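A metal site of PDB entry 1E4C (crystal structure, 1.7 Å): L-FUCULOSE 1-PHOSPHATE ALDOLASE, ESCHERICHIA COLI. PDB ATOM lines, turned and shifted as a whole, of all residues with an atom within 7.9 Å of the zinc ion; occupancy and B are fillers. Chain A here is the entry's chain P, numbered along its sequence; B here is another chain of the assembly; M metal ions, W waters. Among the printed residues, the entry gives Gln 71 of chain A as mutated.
ND2 of Asn 29 lies within hydrogen-bond range of OE1 of Glu 73 (3.0 Å).
A ring nitrogen (ND1) of His 92 is in hydrogen-bond range of the backbone carbonyl oxygen (O) of Leu 157 (2.8 Å).
OH of Tyr 113 of chain B sits close to NE2 of His 155 (3.4 Å).
The backbone NH (N) of His 92 sits at hydrogen-bond distance from the backbone carbonyl oxygen (O) of Asn 29.
The side-chain hydroxyl (OH) of Tyr 113 of chain B lies close to a ring nitrogen (NE2) of His 94 (3.5 Å).
The backbone carbonyl oxygen (O) of His 155 lies within hydrogen-bond range of a ring nitrogen (NE2) of His 112 of chain B (2.8 Å).
N of Glu 73 lies within hydrogen-bond range of OE1 of Gln 71 (2.8 Å).
Tyr 113 of chain B touches the zinc ion.
Of the 22 residues printed, 5 come within 4 Å of the zinc ion.
The nearest printed residue that does not touch the zinc ion is Ala 27 (4.1 Å).
The zinc ion is bound by NE2 of His 92 (2.1 Å), NE2 of His 155 (2.1 Å), NE2 of His 94 (2.1 Å), water W1 (2.1 Å) and OE2 of Glu 73 (2.2 Å).
Water W1 lies within hydrogen-bond range of the side-chain carboxylate of Glu 73 (2.5 Å) and the backbone carbonyl oxygen of Ala 27 (2.7 Å).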
ATOM      1  N   THR A  26     -14.444   2.025   6.673  1.00  0.00           N
ATOM      2  CA  THR A  26     -15.882   2.217   6.525  1.00  0.00           C
ATOM      3  C   THR A  26     -16.712   1.368   7.484  1.00  0.00           C
ATOM      4  O   THR A  26     -17.902   1.175   7.235  1.00  0.00           O
ATOM      5  CB  THR A  26     -16.296   1.853   5.075  1.00  0.00           C
ATOM      6  OG1 THR A  26     -15.871   0.497   4.837  1.00  0.00           O
ATOM      7  CG2 THR A  26     -15.642   2.786   4.057  1.00  0.00           C
ATOM      8  N   ALA A  27     -16.094   0.926   8.571  1.00  0.00           N
ATOM      9  CA  ALA A  27     -16.772   0.045   9.516  1.00  0.00           C
ATOM     10  C   ALA A  27     -17.807   0.741  10.380  1.00  0.00           C
ATOM     11  O   ALA A  27     -18.821   0.135  10.767  1.00  0.00           O
ATOM     12  CB  ALA A  27     -15.715  -0.583  10.438  1.00  0.00           C
ATOM     13  N   GLY A  28     -17.565   1.990  10.758  1.00  0.00           N
ATOM     14  CA  GLY A  28     -18.468   2.682  11.692  1.00  0.00           C
ATOM     15  C   GLY A  28     -19.634   3.369  11.031  1.00  0.00           C
ATOM     16  O   GLY A  28     -19.663   3.648   9.829  1.00  0.00           O
ATOM     17  N   ASN A  29     -20.684   3.631  11.817  1.00  0.00           N
ATOM     18  CA  ASN A  29     -21.857   4.354  11.329  1.00  0.00           C
ATOM     19  C   ASN A  29     -22.501   4.982  12.571  1.00  0.00           C
ATOM     20  O   ASN A  29     -22.315   4.542  13.717  1.00  0.00           O
ATOM     21  CB  ASN A  29     -22.891   3.544  10.565  1.00  0.00           C
ATOM     22  CG  ASN A  29     -23.049   2.113  11.022  1.00  0.00           C
ATOM     23  OD1 ASN A  29     -23.615   1.866  12.081  1.00  0.00           O
ATOM     24  ND2 ASN A  29     -22.518   1.187  10.222  1.00  0.00           N
ATOM     25  N   GLN A  71     -27.677   1.651   3.831  1.00  0.00           N
ATOM     26  CA  GLN A  71     -26.961   1.499   5.105  1.00  0.00           C
ATOM     27  C   GLN A  71     -27.358   0.087   5.561  1.00  0.00           C
ATOM     28  O   GLN A  71     -28.406  -0.126   6.156  1.00  0.00           O
ATOM     29  CB  GLN A  71     -27.237   2.543   6.152  1.00  0.00           C
ATOM     30  CG  GLN A  71     -26.719   2.241   7.556  1.00  0.00           C
ATOM     31  CD  GLN A  71     -25.291   1.738   7.560  1.00  0.00           C
ATOM     32  OE1 GLN A  71     -25.066   0.525   7.678  1.00  0.00           O
ATOM     33  NE2 GLN A  71     -24.319   2.632   7.393  1.00  0.00           N
ATOM     34  N   SER A  72     -26.514  -0.894   5.271  1.00  0.00           N
ATOM     35  CA  SER A  72     -26.802  -2.294   5.524  1.00  0.00           C
ATOM     36  C   SER A  72     -26.994  -2.657   6.977  1.00  0.00           C
ATOM     37  O   SER A  72     -27.577  -3.721   7.229  1.00  0.00           O
ATOM     38  CB  SER A  72     -25.746  -3.177   4.849  1.00  0.00           C
ATOM     39  OG  SER A  72     -24.512  -3.077   5.534  1.00  0.00           O
ATOM     40  N   GLU A  73     -26.553  -1.835   7.935  1.00  0.00           N
ATOM     41  CA  GLU A  73     -26.766  -2.132   9.342  1.00  0.00           C
ATOM     42  C   GLU A  73     -27.827  -1.244   9.980  1.00  0.00           C
ATOM     43  O   GLU A  73     -27.937  -1.174  11.215  1.00  0.00           O
ATOM     44  CB  GLU A  73     -25.436  -1.947  10.103  1.00  0.00           C
ATOM     45  CG  GLU A  73     -24.499  -3.121   9.789  1.00  0.00           C
ATOM     46  CD  GLU A  73     -23.079  -2.816  10.204  1.00  0.00           C
ATOM     47  OE1 GLU A  73     -22.535  -1.782   9.798  1.00  0.00           O
ATOM     48  OE2 GLU A  73     -22.526  -3.641  10.951  1.00  0.00           O
ATOM     49  N   PHE A  76     -30.286  -2.492  13.226  1.00  0.00           N
ATOM     50  CA  PHE A  76     -29.979  -2.505  14.660  1.00  0.00           C
ATOM     51  C   PHE A  76     -29.944  -1.102  15.253  1.00  0.00           C
ATOM     52  O   PHE A  76     -30.050  -0.963  16.470  1.00  0.00           O
ATOM     53  CB  PHE A  76     -28.798  -3.382  15.006  1.00  0.00           C
ATOM     54  CG  PHE A  76     -27.414  -3.085  14.526  1.00  0.00           C
ATOM     55  CD1 PHE A  76     -26.883  -1.817  14.506  1.00  0.00           C
ATOM     56  CD2 PHE A  76     -26.616  -4.143  14.101  1.00  0.00           C
ATOM     57  CE1 PHE A  76     -25.580  -1.583  14.068  1.00  0.00           C
ATOM     58  CE2 PHE A  76     -25.320  -3.914  13.651  1.00  0.00           C
ATOM     59  CZ  PHE A  76     -24.804  -2.639  13.648  1.00  0.00           C
ATOM     60  N   HIS A  92     -21.991   3.125  16.237  1.00  0.00           N
ATOM     61  CA  HIS A  92     -21.535   1.745  16.017  1.00  0.00           C
ATOM     62  C   HIS A  92     -20.117   1.764  15.457  1.00  0.00           C
ATOM     63  O   HIS A  92     -19.828   2.563  14.574  1.00  0.00           O
ATOM     64  CB  HIS A  92     -22.431   1.015  15.004  1.00  0.00           C
ATOM     65  CG  HIS A  92     -21.909  -0.318  14.565  1.00  0.00           C
ATOM     66  ND1 HIS A  92     -21.691  -1.354  15.447  1.00  0.00           N
ATOM     67  CD2 HIS A  92     -21.552  -0.749  13.331  1.00  0.00           C
ATOM     68  CE1 HIS A  92     -21.224  -2.391  14.749  1.00  0.00           C
ATOM     69  NE2 HIS A  92     -21.134  -2.061  13.475  1.00  0.00           N
ATOM     70  N   ASN A  93     -19.233   0.898  15.958  1.00  0.00           N
ATOM     71  CA  ASN A  93     -17.911   0.832  15.322  1.00  0.00           C
ATOM     72  C   ASN A  93     -17.349  -0.560  15.584  1.00  0.00           C
ATOM     73  O   ASN A  93     -17.997  -1.367  16.255  1.00  0.00           O
ATOM     74  CB  ASN A  93     -16.971   1.914  15.828  1.00  0.00           C
ATOM     75  CG  ASN A  93     -16.759   1.846  17.319  1.00  0.00           C
ATOM     76  OD1 ASN A  93     -16.498   0.787  17.884  1.00  0.00           O
ATOM     77  ND2 ASN A  93     -16.848   3.003  17.992  1.00  0.00           N
ATOM     78  N   HIS A  94     -16.190  -0.837  14.990  1.00  0.00           N
ATOM     79  CA  HIS A  94     -15.514  -2.120  15.164  1.00  0.00           C
ATOM     80  C   HIS A  94     -14.182  -1.797  15.864  1.00  0.00           C
ATOM     81  O   HIS A  94     -13.141  -2.281  15.457  1.00  0.00           O
ATOM     82  CB  HIS A  94     -15.293  -2.859  13.853  1.00  0.00           C
ATOM     83  CG  HIS A  94     -16.515  -3.186  13.060  1.00  0.00           C
ATOM     84  ND1 HIS A  94     -16.388  -3.814  11.833  1.00  0.00           N
ATOM     85  CD2 HIS A  94     -17.851  -3.040  13.274  1.00  0.00           C
ATOM     86  CE1 HIS A  94     -17.602  -3.997  11.326  1.00  0.00           C
ATOM     87  NE2 HIS A  94     -18.508  -3.539  12.184  1.00  0.00           N
ATOM     88  N   PHE A 131     -24.984  -9.625  10.081  1.00  0.00           N
ATOM     89  CA  PHE A 131     -25.319  -8.208  10.012  1.00  0.00           C
ATOM     90  C   PHE A 131     -26.534  -8.002   9.104  1.00  0.00           C
ATOM     91  O   PHE A 131     -26.760  -8.738   8.140  1.00  0.00           O
ATOM     92  CB  PHE A 131     -24.160  -7.361   9.486  1.00  0.00           C
ATOM     93  CG  PHE A 131     -23.790  -7.519   8.030  1.00  0.00           C
ATOM     94  CD1 PHE A 131     -22.930  -8.522   7.619  1.00  0.00           C
ATOM     95  CD2 PHE A 131     -24.308  -6.657   7.072  1.00  0.00           C
ATOM     96  CE1 PHE A 131     -22.588  -8.664   6.296  1.00  0.00           C
ATOM     97  CE2 PHE A 131     -23.964  -6.794   5.735  1.00  0.00           C
ATOM     98  CZ  PHE A 131     -23.109  -7.798   5.346  1.00  0.00           C
ATOM     99  N   LEU A 136     -30.254 -10.405  14.463  1.00  0.00           N
ATOM    100  CA  LEU A 136     -29.251  -9.557  15.147  1.00  0.00           C
ATOM    101  C   LEU A 136     -29.943  -8.404  15.859  1.00  0.00           C
ATOM    102  O   LEU A 136     -29.609  -8.085  17.005  1.00  0.00           O
ATOM    103  CB  LEU A 136     -28.192  -9.058  14.167  1.00  0.00           C
ATOM    104  CG  LEU A 136     -27.074  -8.186  14.768  1.00  0.00           C
ATOM    105  CD1 LEU A 136     -26.349  -8.908  15.884  1.00  0.00           C
ATOM    106  CD2 LEU A 136     -26.107  -7.748  13.668  1.00  0.00           C
ATOM    107  N   LEU A 152     -20.985  -6.858  20.364  1.00  0.00           N
ATOM    108  CA  LEU A 152     -21.664  -7.730  19.402  1.00  0.00           C
ATOM    109  C   LEU A 152     -20.674  -8.855  19.045  1.00  0.00           C
ATOM    110  O   LEU A 152     -19.631  -8.557  18.467  1.00  0.00           O
ATOM    111  CB  LEU A 152     -22.067  -6.939  18.156  1.00  0.00           C
ATOM    112  CG  LEU A 152     -23.299  -6.050  18.344  1.00  0.00           C
ATOM    113  CD1 LEU A 152     -22.908  -4.716  18.957  1.00  0.00           C
ATOM    114  CD2 LEU A 152     -24.027  -5.830  17.025  1.00  0.00           C
ATOM    115  N   HIS A 154     -18.176 -11.443  17.590  1.00  0.00           N
ATOM    116  CA  HIS A 154     -17.516 -11.485  16.302  1.00  0.00           C
ATOM    117  C   HIS A 154     -17.819 -10.263  15.451  1.00  0.00           C
ATOM    118  O   HIS A 154     -17.826 -10.382  14.220  1.00  0.00           O
ATOM    119  CB  HIS A 154     -17.874 -12.760  15.524  1.00  0.00           C
ATOM    120  CG  HIS A 154     -17.322 -14.020  16.119  1.00  0.00           C
ATOM    121  ND1 HIS A 154     -15.980 -14.351  16.124  1.00  0.00           N
ATOM    122  CD2 HIS A 154     -17.971 -15.056  16.701  1.00  0.00           C
ATOM    123  CE1 HIS A 154     -15.841 -15.532  16.725  1.00  0.00           C
ATOM    124  NE2 HIS A 154     -17.022 -15.991  17.070  1.00  0.00           N
ATOM    125  N   HIS A 155     -18.037  -9.093  16.096  1.00  0.00           N
ATOM    126  CA  HIS A 155     -18.455  -7.956  15.265  1.00  0.00           C
ATOM    127  C   HIS A 155     -17.931  -6.628  15.780  1.00  0.00           C
ATOM    128  O   HIS A 155     -17.107  -6.012  15.081  1.00  0.00           O
ATOM    129  CB  HIS A 155     -19.987  -7.974  15.176  1.00  0.00           C
ATOM    130  CG  HIS A 155     -20.548  -6.960  14.218  1.00  0.00           C
ATOM    131  ND1 HIS A 155     -21.744  -7.145  13.559  1.00  0.00           N
ATOM    132  CD2 HIS A 155     -20.078  -5.764  13.811  1.00  0.00           C
ATOM    133  CE1 HIS A 155     -21.955  -6.083  12.780  1.00  0.00           C
ATOM    134  NE2 HIS A 155     -20.953  -5.223  12.918  1.00  0.00           N
ATOM    135  N   GLY A 156     -18.401  -6.139  16.915  1.00  0.00           N
ATOM    136  CA  GLY A 156     -17.954  -4.803  17.339  1.00  0.00           C
ATOM    137  C   GLY A 156     -18.801  -4.283  18.488  1.00  0.00           C
ATOM    138  O   GLY A 156     -19.154  -5.029  19.398  1.00  0.00           O
ATOM    139  N   LEU A 157     -19.084  -2.991  18.454  1.00  0.00           N
ATOM    140  CA  LEU A 157     -19.752  -2.295  19.558  1.00  0.00           C
ATOM    141  C   LEU A 157     -20.933  -1.457  19.129  1.00  0.00           C
ATOM    142  O   LEU A 157     -20.910  -0.806  18.077  1.00  0.00           O
ATOM    143  CB  LEU A 157     -18.688  -1.396  20.201  1.00  0.00           C
ATOM    144  CG  LEU A 157     -18.989  -0.402  21.309  1.00  0.00           C
ATOM    145  CD1 LEU A 157     -19.631   0.880  20.795  1.00  0.00           C
ATOM    146  CD2 LEU A 157     -19.823  -1.002  22.425  1.00  0.00           C
ATOM    147  N   ILE A 158     -21.956  -1.328  19.982  1.00  0.00           N
ATOM    148  CA  ILE A 158     -23.040  -0.377  19.831  1.00  0.00           C
ATOM    149  C   ILE A 158     -23.158   0.409  21.159  1.00  0.00           C
ATOM    150  O   ILE A 158     -23.143  -0.182  22.238  1.00  0.00           O
ATOM    151  CB  ILE A 158     -24.408  -1.004  19.552  1.00  0.00           C
ATOM    152  CG1 ILE A 158     -24.489  -1.454  18.091  1.00  0.00           C
ATOM    153  CG2 ILE A 158     -25.555  -0.059  19.894  1.00  0.00           C
ATOM    154  CD1 ILE A 158     -24.541  -0.337  17.080  1.00  0.00           C
ATOM    155  N   HIS B 112     -13.673 -13.001  12.569  1.00  0.00           N
ATOM    156  CA  HIS B 112     -14.532 -11.840  12.368  1.00  0.00           C
ATOM    157  C   HIS B 112     -15.138 -11.936  10.975  1.00  0.00           C
ATOM    158  O   HIS B 112     -14.470 -12.478  10.082  1.00  0.00           O
ATOM    159  CB  HIS B 112     -13.710 -10.564  12.543  1.00  0.00           C
ATOM    160  CG  HIS B 112     -14.544  -9.329  12.643  1.00  0.00           C
ATOM    161  ND1 HIS B 112     -15.130  -8.745  11.545  1.00  0.00           N
ATOM    162  CD2 HIS B 112     -14.889  -8.562  13.719  1.00  0.00           C
ATOM    163  CE1 HIS B 112     -15.828  -7.681  11.925  1.00  0.00           C
ATOM    164  NE2 HIS B 112     -15.675  -7.537  13.238  1.00  0.00           N
ATOM    165  N   TYR B 113     -16.368 -11.454  10.806  1.00  0.00           N
ATOM    166  CA  TYR B 113     -17.019 -11.567   9.499  1.00  0.00           C
ATOM    167  C   TYR B 113     -16.347 -10.793   8.398  1.00  0.00           C
ATOM    168  O   TYR B 113     -16.481 -11.195   7.239  1.00  0.00           O
ATOM    169  CB  TYR B 113     -18.511 -11.229   9.576  1.00  0.00           C
ATOM    170  CG  TYR B 113     -18.849  -9.752   9.636  1.00  0.00           C
ATOM    171  CD1 TYR B 113     -19.063  -9.031   8.481  1.00  0.00           C
ATOM    172  CD2 TYR B 113     -18.977  -9.105  10.855  1.00  0.00           C
ATOM    173  CE1 TYR B 113     -19.379  -7.681   8.525  1.00  0.00           C
ATOM    174  CE2 TYR B 113     -19.295  -7.752  10.908  1.00  0.00           C
ATOM    175  CZ  TYR B 113     -19.504  -7.057   9.743  1.00  0.00           C
ATOM    176  OH  TYR B 113     -19.819  -5.716   9.792  1.00  0.00           O
ATOM    177  N   MET B 114     -15.539  -9.770   8.672  1.00  0.00           N
ATOM    178  CA  MET B 114     -14.833  -9.011   7.677  1.00  0.00           C
ATOM    179  C   MET B 114     -13.693  -9.782   7.019  1.00  0.00           C
ATOM    180  O   MET B 114     -13.172  -9.294   6.009  1.00  0.00           O
ATOM    181  CB  MET B 114     -14.277  -7.707   8.256  1.00  0.00           C
ATOM    182  CG  MET B 114     -15.365  -6.681   8.553  1.00  0.00           C
ATOM    183  SD  MET B 114     -16.116  -6.080   7.012  1.00  0.00           S
ATOM    184  CE  MET B 114     -14.675  -5.393   6.202  1.00  0.00           C
HETATM  185 ZN    ZN M   1     -20.594  -3.395  11.961  1.00  0.00          ZN
HETATM  186  O   HOH W   1     -20.133  -2.147  10.313  1.00  0.00           O
